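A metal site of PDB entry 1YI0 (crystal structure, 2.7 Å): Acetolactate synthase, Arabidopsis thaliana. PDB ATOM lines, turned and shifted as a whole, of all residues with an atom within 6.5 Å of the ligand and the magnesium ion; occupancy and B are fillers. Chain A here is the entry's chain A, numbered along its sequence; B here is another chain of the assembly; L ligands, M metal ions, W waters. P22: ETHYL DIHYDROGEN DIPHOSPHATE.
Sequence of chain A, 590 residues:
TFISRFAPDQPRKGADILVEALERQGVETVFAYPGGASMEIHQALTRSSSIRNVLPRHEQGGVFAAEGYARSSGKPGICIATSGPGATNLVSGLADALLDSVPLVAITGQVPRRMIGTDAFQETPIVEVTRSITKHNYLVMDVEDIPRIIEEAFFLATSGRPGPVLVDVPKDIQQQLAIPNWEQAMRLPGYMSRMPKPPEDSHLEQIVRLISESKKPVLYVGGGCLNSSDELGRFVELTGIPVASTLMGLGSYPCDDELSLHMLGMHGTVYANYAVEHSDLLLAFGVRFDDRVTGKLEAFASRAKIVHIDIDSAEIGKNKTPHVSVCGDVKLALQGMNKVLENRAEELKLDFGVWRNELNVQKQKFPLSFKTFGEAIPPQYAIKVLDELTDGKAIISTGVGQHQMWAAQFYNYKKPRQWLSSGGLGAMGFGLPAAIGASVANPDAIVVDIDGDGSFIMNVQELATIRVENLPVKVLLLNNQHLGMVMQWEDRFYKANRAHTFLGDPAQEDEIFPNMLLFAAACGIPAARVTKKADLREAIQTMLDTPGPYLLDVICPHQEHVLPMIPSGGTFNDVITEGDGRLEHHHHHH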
ATOM      1  N   GLY A 399      18.021  16.622  21.507  1.00  0.00           N
ATOM      2  CA  GLY A 399      17.276  16.554  20.271  1.00  0.00           C
ATOM      3  C   GLY A 399      15.911  16.079  20.716  1.00  0.00           C
ATOM      4  O   GLY A 399      15.524  16.278  21.870  1.00  0.00           O
ATOM      5  N   VAL A 400      15.172  15.439  19.823  1.00  0.00           N
ATOM      6  CA  VAL A 400      13.845  14.953  20.148  1.00  0.00           C
ATOM      7  C   VAL A 400      13.787  13.443  19.915  1.00  0.00           C
ATOM      8  O   VAL A 400      14.343  12.933  18.941  1.00  0.00           O
ATOM      9  CB  VAL A 400      12.775  15.662  19.266  1.00  0.00           C
ATOM     10  CG1 VAL A 400      11.415  15.033  19.490  1.00  0.00           C
ATOM     11  CG2 VAL A 400      12.737  17.144  19.602  1.00  0.00           C
ATOM     12  N   GLY A 401      13.135  12.730  20.824  1.00  0.00           N
ATOM     13  CA  GLY A 401      13.031  11.289  20.685  1.00  0.00           C
ATOM     14  C   GLY A 401      13.353  10.563  21.982  1.00  0.00           C
ATOM     15  O   GLY A 401      13.224  11.127  23.073  1.00  0.00           O
ATOM     16  N   GLN A 402      13.770   9.306  21.859  1.00  0.00           N
ATOM     17  CA  GLN A 402      14.093   8.488  23.020  1.00  0.00           C
ATOM     18  C   GLN A 402      15.203   9.085  23.863  1.00  0.00           C
ATOM     19  O   GLN A 402      15.072   9.190  25.073  1.00  0.00           O
ATOM     20  CB  GLN A 402      14.498   7.076  22.588  1.00  0.00           C
ATOM     21  CG  GLN A 402      13.434   6.292  21.852  1.00  0.00           C
ATOM     22  CD  GLN A 402      13.899   4.887  21.493  1.00  0.00           C
ATOM     23  OE1 GLN A 402      14.969   4.701  20.909  1.00  0.00           O
ATOM     24  NE2 GLN A 402      13.090   3.885  21.843  1.00  0.00           N
ATOM     25  N   HIS A 403      16.295   9.479  23.223  1.00  0.00           N
ATOM     26  CA  HIS A 403      17.411  10.047  23.968  1.00  0.00           C
ATOM     27  C   HIS A 403      16.951  11.244  24.787  1.00  0.00           C
ATOM     28  O   HIS A 403      17.385  11.444  25.925  1.00  0.00           O
ATOM     29  CB  HIS A 403      18.556  10.470  23.031  1.00  0.00           C
ATOM     30  CG  HIS A 403      18.246  11.652  22.166  1.00  0.00           C
ATOM     31  ND1 HIS A 403      17.398  11.575  21.079  1.00  0.00           N
ATOM     32  CD2 HIS A 403      18.689  12.926  22.211  1.00  0.00           C
ATOM     33  CE1 HIS A 403      17.330  12.756  20.488  1.00  0.00           C
ATOM     34  NE2 HIS A 403      18.110  13.594  21.154  1.00  0.00           N
ATOM     35  N   GLN A 404      16.046  12.034  24.209  1.00  0.00           N
ATOM     36  CA  GLN A 404      15.497  13.199  24.883  1.00  0.00           C
ATOM     37  C   GLN A 404      14.799  12.741  26.146  1.00  0.00           C
ATOM     38  O   GLN A 404      15.026  13.295  27.224  1.00  0.00           O
ATOM     39  CB  GLN A 404      14.525  13.924  23.947  1.00  0.00           C
ATOM     40  CG  GLN A 404      13.675  14.984  24.615  1.00  0.00           C
ATOM     41  CD  GLN A 404      12.701  15.607  23.634  1.00  0.00           C
ATOM     42  OE1 GLN A 404      12.127  14.921  22.795  1.00  0.00           O
ATOM     43  NE2 GLN A 404      12.496  16.916  23.749  1.00  0.00           N
ATOM     44  N   TRP A 406      15.263   9.956  27.806  1.00  0.00           N
ATOM     45  CA  TRP A 406      16.238   9.471  28.767  1.00  0.00           C
ATOM     46  C   TRP A 406      17.009  10.615  29.400  1.00  0.00           C
ATOM     47  O   TRP A 406      17.286  10.598  30.599  1.00  0.00           O
ATOM     48  CB  TRP A 406      17.185   8.452  28.124  1.00  0.00           C
ATOM     49  CG  TRP A 406      16.491   7.175  27.730  1.00  0.00           C
ATOM     50  CD1 TRP A 406      15.551   6.500  28.460  1.00  0.00           C
ATOM     51  CD2 TRP A 406      16.642   6.468  26.504  1.00  0.00           C
ATOM     52  NE1 TRP A 406      15.094   5.410  27.750  1.00  0.00           N
ATOM     53  CE2 TRP A 406      15.748   5.368  26.549  1.00  0.00           C
ATOM     54  CE3 TRP A 406      17.446   6.644  25.366  1.00  0.00           C
ATOM     55  CZ2 TRP A 406      15.635   4.448  25.483  1.00  0.00           C
ATOM     56  CZ3 TRP A 406      17.331   5.731  24.312  1.00  0.00           C
ATOM     57  CH2 TRP A 406      16.424   4.656  24.381  1.00  0.00           C
ATOM     58  N   MET A 428      13.290  18.320  15.862  1.00  0.00           N
ATOM     59  CA  MET A 428      14.594  17.669  15.784  1.00  0.00           C
ATOM     60  C   MET A 428      15.653  18.669  15.314  1.00  0.00           C
ATOM     61  O   MET A 428      15.335  19.659  14.651  1.00  0.00           O
ATOM     62  CB  MET A 428      14.529  16.491  14.820  1.00  0.00           C
ATOM     63  CG  MET A 428      13.836  15.253  15.369  1.00  0.00           C
ATOM     64  SD  MET A 428      13.723  13.952  14.130  1.00  0.00           S
ATOM     65  CE  MET A 428      15.481  13.543  13.896  1.00  0.00           C
ATOM     66  N   ASP A 451      22.415  14.278  22.132  1.00  0.00           N
ATOM     67  CA  ASP A 451      21.694  14.154  20.876  1.00  0.00           C
ATOM     68  C   ASP A 451      21.451  12.737  20.380  1.00  0.00           C
ATOM     69  O   ASP A 451      21.978  11.761  20.931  1.00  0.00           O
ATOM     70  CB  ASP A 451      22.454  14.913  19.786  1.00  0.00           C
ATOM     71  CG  ASP A 451      21.597  15.932  19.073  1.00  0.00           C
ATOM     72  OD1 ASP A 451      20.389  15.684  18.921  1.00  0.00           O
ATOM     73  OD2 ASP A 451      22.141  16.976  18.663  1.00  0.00           O
ATOM     74  N   GLY A 452      20.638  12.642  19.335  1.00  0.00           N
ATOM     75  CA  GLY A 452      20.332  11.375  18.709  1.00  0.00           C
ATOM     76  C   GLY A 452      21.009  11.442  17.350  1.00  0.00           C
ATOM     77  O   GLY A 452      21.297  12.539  16.884  1.00  0.00           O
ATOM     78  N   ASP A 453      21.257  10.304  16.722  1.00  0.00           N
ATOM     79  CA  ASP A 453      21.936  10.327  15.425  1.00  0.00           C
ATOM     80  C   ASP A 453      21.067  10.966  14.349  1.00  0.00           C
ATOM     81  O   ASP A 453      21.582  11.584  13.419  1.00  0.00           O
ATOM     82  CB  ASP A 453      22.379   8.913  15.009  1.00  0.00           C
ATOM     83  CG  ASP A 453      21.254   7.898  15.039  1.00  0.00           C
ATOM     84  OD1 ASP A 453      20.535   7.832  16.071  1.00  0.00           O
ATOM     85  OD2 ASP A 453      21.077   7.162  14.050  1.00  0.00           O
ATOM     86  N   GLY A 454      19.742  10.839  14.499  1.00  0.00           N
ATOM     87  CA  GLY A 454      18.848  11.443  13.526  1.00  0.00           C
ATOM     88  C   GLY A 454      18.784  12.951  13.698  1.00  0.00           C
ATOM     89  O   GLY A 454      18.909  13.704  12.732  1.00  0.00           O
ATOM     90  N   SER A 455      18.603  13.406  14.942  1.00  0.00           N
ATOM     91  CA  SER A 455      18.509  14.819  15.254  1.00  0.00           C
ATOM     92  C   SER A 455      19.818  15.549  15.026  1.00  0.00           C
ATOM     93  O   SER A 455      19.842  16.657  14.504  1.00  0.00           O
ATOM     94  CB  SER A 455      18.077  15.028  16.714  1.00  0.00           C
ATOM     95  OG  SER A 455      16.793  14.500  16.962  1.00  0.00           O
ATOM     96  N   PHE A 456      20.919  14.911  15.430  1.00  0.00           N
ATOM     97  CA  PHE A 456      22.225  15.526  15.300  1.00  0.00           C
ATOM     98  C   PHE A 456      22.577  15.885  13.858  1.00  0.00           C
ATOM     99  O   PHE A 456      23.081  16.970  13.577  1.00  0.00           O
ATOM    100  CB  PHE A 456      23.307  14.587  15.847  1.00  0.00           C
ATOM    101  CG  PHE A 456      24.702  15.140  15.736  1.00  0.00           C
ATOM    102  CD1 PHE A 456      25.134  16.183  16.555  1.00  0.00           C
ATOM    103  CD2 PHE A 456      25.597  14.617  14.798  1.00  0.00           C
ATOM    104  CE1 PHE A 456      26.426  16.696  16.461  1.00  0.00           C
ATOM    105  CE2 PHE A 456      26.901  15.135  14.686  1.00  0.00           C
ATOM    106  CZ  PHE A 456      27.320  16.174  15.523  1.00  0.00           C
ATOM    107  N   LEU A 478      24.046   9.841  21.390  1.00  0.00           N
ATOM    108  CA  LEU A 478      23.548   8.493  21.651  1.00  0.00           C
ATOM    109  C   LEU A 478      23.139   7.913  20.301  1.00  0.00           C
ATOM    110  O   LEU A 478      21.987   8.016  19.887  1.00  0.00           O
ATOM    111  CB  LEU A 478      22.336   8.528  22.593  1.00  0.00           C
ATOM    112  CG  LEU A 478      22.609   9.149  23.964  1.00  0.00           C
ATOM    113  CD1 LEU A 478      21.385   8.977  24.865  1.00  0.00           C
ATOM    114  CD2 LEU A 478      23.829   8.487  24.587  1.00  0.00           C
ATOM    115  N   ASN A 479      24.106   7.290  19.630  1.00  0.00           N
ATOM    116  CA  ASN A 479      23.886   6.733  18.303  1.00  0.00           C
ATOM    117  C   ASN A 479      23.243   5.342  18.326  1.00  0.00           C
ATOM    118  O   ASN A 479      23.853   4.371  18.786  1.00  0.00           O
ATOM    119  CB  ASN A 479      25.220   6.667  17.569  1.00  0.00           C
ATOM    120  CG  ASN A 479      25.060   6.542  16.073  1.00  0.00           C
ATOM    121  OD1 ASN A 479      24.058   6.013  15.583  1.00  0.00           O
ATOM    122  ND2 ASN A 479      26.064   7.025  15.338  1.00  0.00           N
ATOM    123  N   ASN A 480      22.015   5.237  17.820  1.00  0.00           N
ATOM    124  CA  ASN A 480      21.320   3.954  17.767  1.00  0.00           C
ATOM    125  C   ASN A 480      20.923   3.590  16.325  1.00  0.00           C
ATOM    126  O   ASN A 480      20.107   2.688  16.106  1.00  0.00           O
ATOM    127  CB  ASN A 480      20.092   3.973  18.682  1.00  0.00           C
ATOM    128  CG  ASN A 480      18.950   4.817  18.134  1.00  0.00           C
ATOM    129  OD1 ASN A 480      19.131   5.607  17.196  1.00  0.00           O
ATOM    130  ND2 ASN A 480      17.772   4.667  18.726  1.00  0.00           N
ATOM    131  N   GLN A 481      21.504   4.303  15.354  1.00  0.00           N
ATOM    132  CA  GLN A 481      21.252   4.052  13.940  1.00  0.00           C
ATOM    133  C   GLN A 481      19.806   4.125  13.465  1.00  0.00           C
ATOM    134  O   GLN A 481      19.516   3.791  12.316  1.00  0.00           O
ATOM    135  CB  GLN A 481      21.811   2.676  13.560  1.00  0.00           C
ATOM    136  CG  GLN A 481      23.301   2.517  13.750  1.00  0.00           C
ATOM    137  CD  GLN A 481      24.109   3.457  12.866  1.00  0.00           C
ATOM    138  OE1 GLN A 481      24.300   4.635  13.184  1.00  0.00           O
ATOM    139  NE2 GLN A 481      24.578   2.939  11.732  1.00  0.00           N
ATOM    140  N   HIS A 482      18.884   4.552  14.325  1.00  0.00           N
ATOM    141  CA  HIS A 482      17.475   4.649  13.934  1.00  0.00           C
ATOM    142  C   HIS A 482      16.789   5.921  14.427  1.00  0.00           C
ATOM    143  O   HIS A 482      17.369   6.726  15.149  1.00  0.00           O
ATOM    144  CB  HIS A 482      16.666   3.473  14.502  1.00  0.00           C
ATOM    145  CG  HIS A 482      16.993   2.135  13.911  1.00  0.00           C
ATOM    146  ND1 HIS A 482      18.190   1.491  14.140  1.00  0.00           N
ATOM    147  CD2 HIS A 482      16.261   1.308  13.120  1.00  0.00           C
ATOM    148  CE1 HIS A 482      18.177   0.331  13.510  1.00  0.00           C
ATOM    149  NE2 HIS A 482      17.028   0.196  12.884  1.00  0.00           N
ATOM    150  N   LEU A 483      15.546   6.074  14.001  1.00  0.00           N
ATOM    151  CA  LEU A 483      14.705   7.170  14.470  1.00  0.00           C
ATOM    152  C   LEU A 483      13.989   6.443  15.605  1.00  0.00           C
ATOM    153  O   LEU A 483      12.842   6.013  15.460  1.00  0.00           O
ATOM    154  CB  LEU A 483      13.718   7.609  13.392  1.00  0.00           C
ATOM    155  CG  LEU A 483      14.309   8.382  12.209  1.00  0.00           C
ATOM    156  CD1 LEU A 483      13.247   8.643  11.171  1.00  0.00           C
ATOM    157  CD2 LEU A 483      14.908   9.683  12.699  1.00  0.00           C
ATOM    158  N   GLY A 484      14.717   6.276  16.700  1.00  0.00           N
ATOM    159  CA  GLY A 484      14.246   5.570  17.885  1.00  0.00           C
ATOM    160  C   GLY A 484      12.795   5.669  18.320  1.00  0.00           C
ATOM    161  O   GLY A 484      12.082   4.659  18.370  1.00  0.00           O
ATOM    162  N   MET A 485      12.357   6.888  18.649  1.00  0.00           N
ATOM    163  CA  MET A 485      10.992   7.069  19.105  1.00  0.00           C
ATOM    164  C   MET A 485       9.974   6.490  18.113  1.00  0.00           C
ATOM    165  O   MET A 485       9.022   5.827  18.522  1.00  0.00           O
ATOM    166  CB  MET A 485      10.717   8.564  19.337  1.00  0.00           C
ATOM    167  CG  MET A 485       9.422   8.859  20.069  1.00  0.00           C
ATOM    168  SD  MET A 485       9.261   7.968  21.630  1.00  0.00           S
ATOM    169  CE  MET A 485      10.050   9.112  22.753  1.00  0.00           C
ATOM    170  N   VAL A 486      10.183   6.724  16.829  1.00  0.00           N
ATOM    171  CA  VAL A 486       9.256   6.192  15.830  1.00  0.00           C
ATOM    172  C   VAL A 486       9.350   4.668  15.731  1.00  0.00           C
ATOM    173  O   VAL A 486       8.321   4.010  15.570  1.00  0.00           O
ATOM    174  CB  VAL A 486       9.488   6.793  14.429  1.00  0.00           C
ATOM    175  CG1 VAL A 486       8.457   6.251  13.454  1.00  0.00           C
ATOM    176  CG2 VAL A 486       9.389   8.292  14.500  1.00  0.00           C
ATOM    177  N   LEU A 503      18.410   4.710   9.891  1.00  0.00           N
ATOM    178  CA  LEU A 503      19.256   5.805   9.413  1.00  0.00           C
ATOM    179  C   LEU A 503      20.625   5.375   8.878  1.00  0.00           C
ATOM    180  O   LEU A 503      21.378   6.204   8.375  1.00  0.00           O
ATOM    181  CB  LEU A 503      19.472   6.821  10.527  1.00  0.00           C
ATOM    182  CG  LEU A 503      18.213   7.437  11.122  1.00  0.00           C
ATOM    183  CD1 LEU A 503      18.575   8.237  12.362  1.00  0.00           C
ATOM    184  CD2 LEU A 503      17.517   8.309  10.096  1.00  0.00           C
ATOM    185  N   TYR B  33       9.783  11.845   5.186  1.00  0.00           N
ATOM    186  CA  TYR B  33      10.498  11.661   6.440  1.00  0.00           C
ATOM    187  C   TYR B  33       9.435  11.369   7.493  1.00  0.00           C
ATOM    188  O   TYR B  33       8.574  12.199   7.772  1.00  0.00           O
ATOM    189  CB  TYR B  33      11.260  12.943   6.783  1.00  0.00           C
ATOM    190  CG  TYR B  33      12.342  12.754   7.820  1.00  0.00           C
ATOM    191  CD1 TYR B  33      13.664  12.489   7.452  1.00  0.00           C
ATOM    192  CD2 TYR B  33      12.039  12.840   9.167  1.00  0.00           C
ATOM    193  CE1 TYR B  33      14.654  12.322   8.419  1.00  0.00           C
ATOM    194  CE2 TYR B  33      13.027  12.681  10.146  1.00  0.00           C
ATOM    195  CZ  TYR B  33      14.331  12.418   9.765  1.00  0.00           C
ATOM    196  OH  TYR B  33      15.288  12.266  10.751  1.00  0.00           O
ATOM    197  N   PRO B  34       9.474  10.168   8.075  1.00  0.00           N
ATOM    198  CA  PRO B  34       8.518   9.724   9.096  1.00  0.00           C
ATOM    199  C   PRO B  34       8.487  10.523  10.392  1.00  0.00           C
ATOM    200  O   PRO B  34       9.509  10.989  10.891  1.00  0.00           O
ATOM    201  CB  PRO B  34       8.906   8.271   9.327  1.00  0.00           C
ATOM    202  CG  PRO B  34      10.383   8.296   9.113  1.00  0.00           C
ATOM    203  CD  PRO B  34      10.518   9.144   7.870  1.00  0.00           C
HETATM  204  C6  P22 L   1      12.994  10.487  15.911  1.00  0.00           C
HETATM  205  C7  P22 L   1      14.304  10.812  16.595  1.00  0.00           C
HETATM  206  O7  P22 L   1      15.373  10.081  16.193  1.00  0.00           O
HETATM  207  PA  P22 L   1      16.821  10.363  16.908  1.00  0.00           P
HETATM  208  O1A P22 L   1      17.285  11.756  16.663  1.00  0.00           O
HETATM  209  O2A P22 L   1      17.831   9.439  16.307  1.00  0.00           O
HETATM  210  O3A P22 L   1      16.757  10.146  18.508  1.00  0.00           O
HETATM  211  PB  P22 L   1      16.092   8.802  19.078  1.00  0.00           P
HETATM  212  O1B P22 L   1      14.604   8.934  19.141  1.00  0.00           O
HETATM  213  O2B P22 L   1      16.491   7.623  18.254  1.00  0.00           O
HETATM  214  O3B P22 L   1      16.616   8.620  20.461  1.00  0.00           O
HETATM  215 MG    MG M   1      18.337   7.572  16.799  1.00  0.00          MG
HETATM  216  O   HOH W   1      19.478   8.129  18.800  1.00  0.00           O
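Water W1 lies within hydrogen-bond range of the backbone carbonyl oxygen (O) of Leu 478 (2.7 Å), an oxygen (O3B) of the ligand (3.3 Å) and the backbone NH (N) of Asp 453 (3.5 Å).
OD2 of Asp 453 sits close to N of Gln 481, at 3.2 Å.
OG of Ser 455 is in hydrogen-bond range of N of Val 400 (3.4 Å).
N of Gly 452 is in hydrogen-bond range of NE2 of His 403, at 3.3 Å.
The backbone NH (N) of Gly 399 lies within hydrogen-bond range of a ring nitrogen (NE2) of His 403, at 3.0 Å.
N of Gly 401 lies within hydrogen-bond range of OE1 of Gln 404.
Merely in contact with the ligand: Val 400 (3.2 Å), Gly 401 (3.2 Å), Met 428 (3.8 Å), Gly 452 (3.7 Å) and Leu 483 (3.4 Å).
Hydrophobic or aromatic side chains within 4 Å of the ligand: His 403, Met 428, Leu 483 and Met 485.
14 residues have an atom within 4 Å of the ligand: Val 400, Gly 401, Gln 402, His 403, Met 428, Gly 452, Asp 453, Gly 454, Ser 455, Asn 480, His 482, Leu 483, Gly 484 and Met 485.
The nearest printed residue that does not touch the ligand is Leu 503 (4.2 Å).
The magnesium ion is bound by O2A of the ligand (2.0 Å), O of His 482 (2.1 Å), OD1 of Asn 480 (2.2 Å), OD1 of Asp 453 (2.3 Å), O2B of the ligand (2.4 Å) and water W1 (2.4 Å).
The magnesium ion has six donor atoms within binding distance.
An oxygen (O2B) of the ligand lies close to the backbone NH (N) of Gly 484, at 2.7 Å.
The backbone NH of Ser 455 sits at hydrogen-bond distance from an oxygen (O1A) of the ligand, at 2.7 Å.
The side-chain hydroxyl (OG) of Ser 455 is in hydrogen-bond range of an oxygen (O1A) of the ligand.
The backbone NH (N) of Gln 402 lies within hydrogen-bond range of an oxygen (O1B) of the ligand, at 2.9 Å.
N of His 403 lies within hydrogen-bond range of O3B of the ligand (2.9 Å).
ND1 of His 403 lies within hydrogen-bond range of O3A of the ligand, 3.0 Å away.
An oxygen (O1A) of the ligand sits at hydrogen-bond distance from the backbone NH of Gly 454.
An oxygen (O1B) of the ligand is in hydrogen-bond range of the backbone NH (N) of Met 485 (3.1 Å).
Residues that only touch the magnesium ion: Gly 484 (3.8 Å).
Of the 26 residues printed, 4 come within 4 Å of the magnesium ion.
The nearest printed residue that does not touch the magnesium ion is Leu 483 (4.2 Å).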
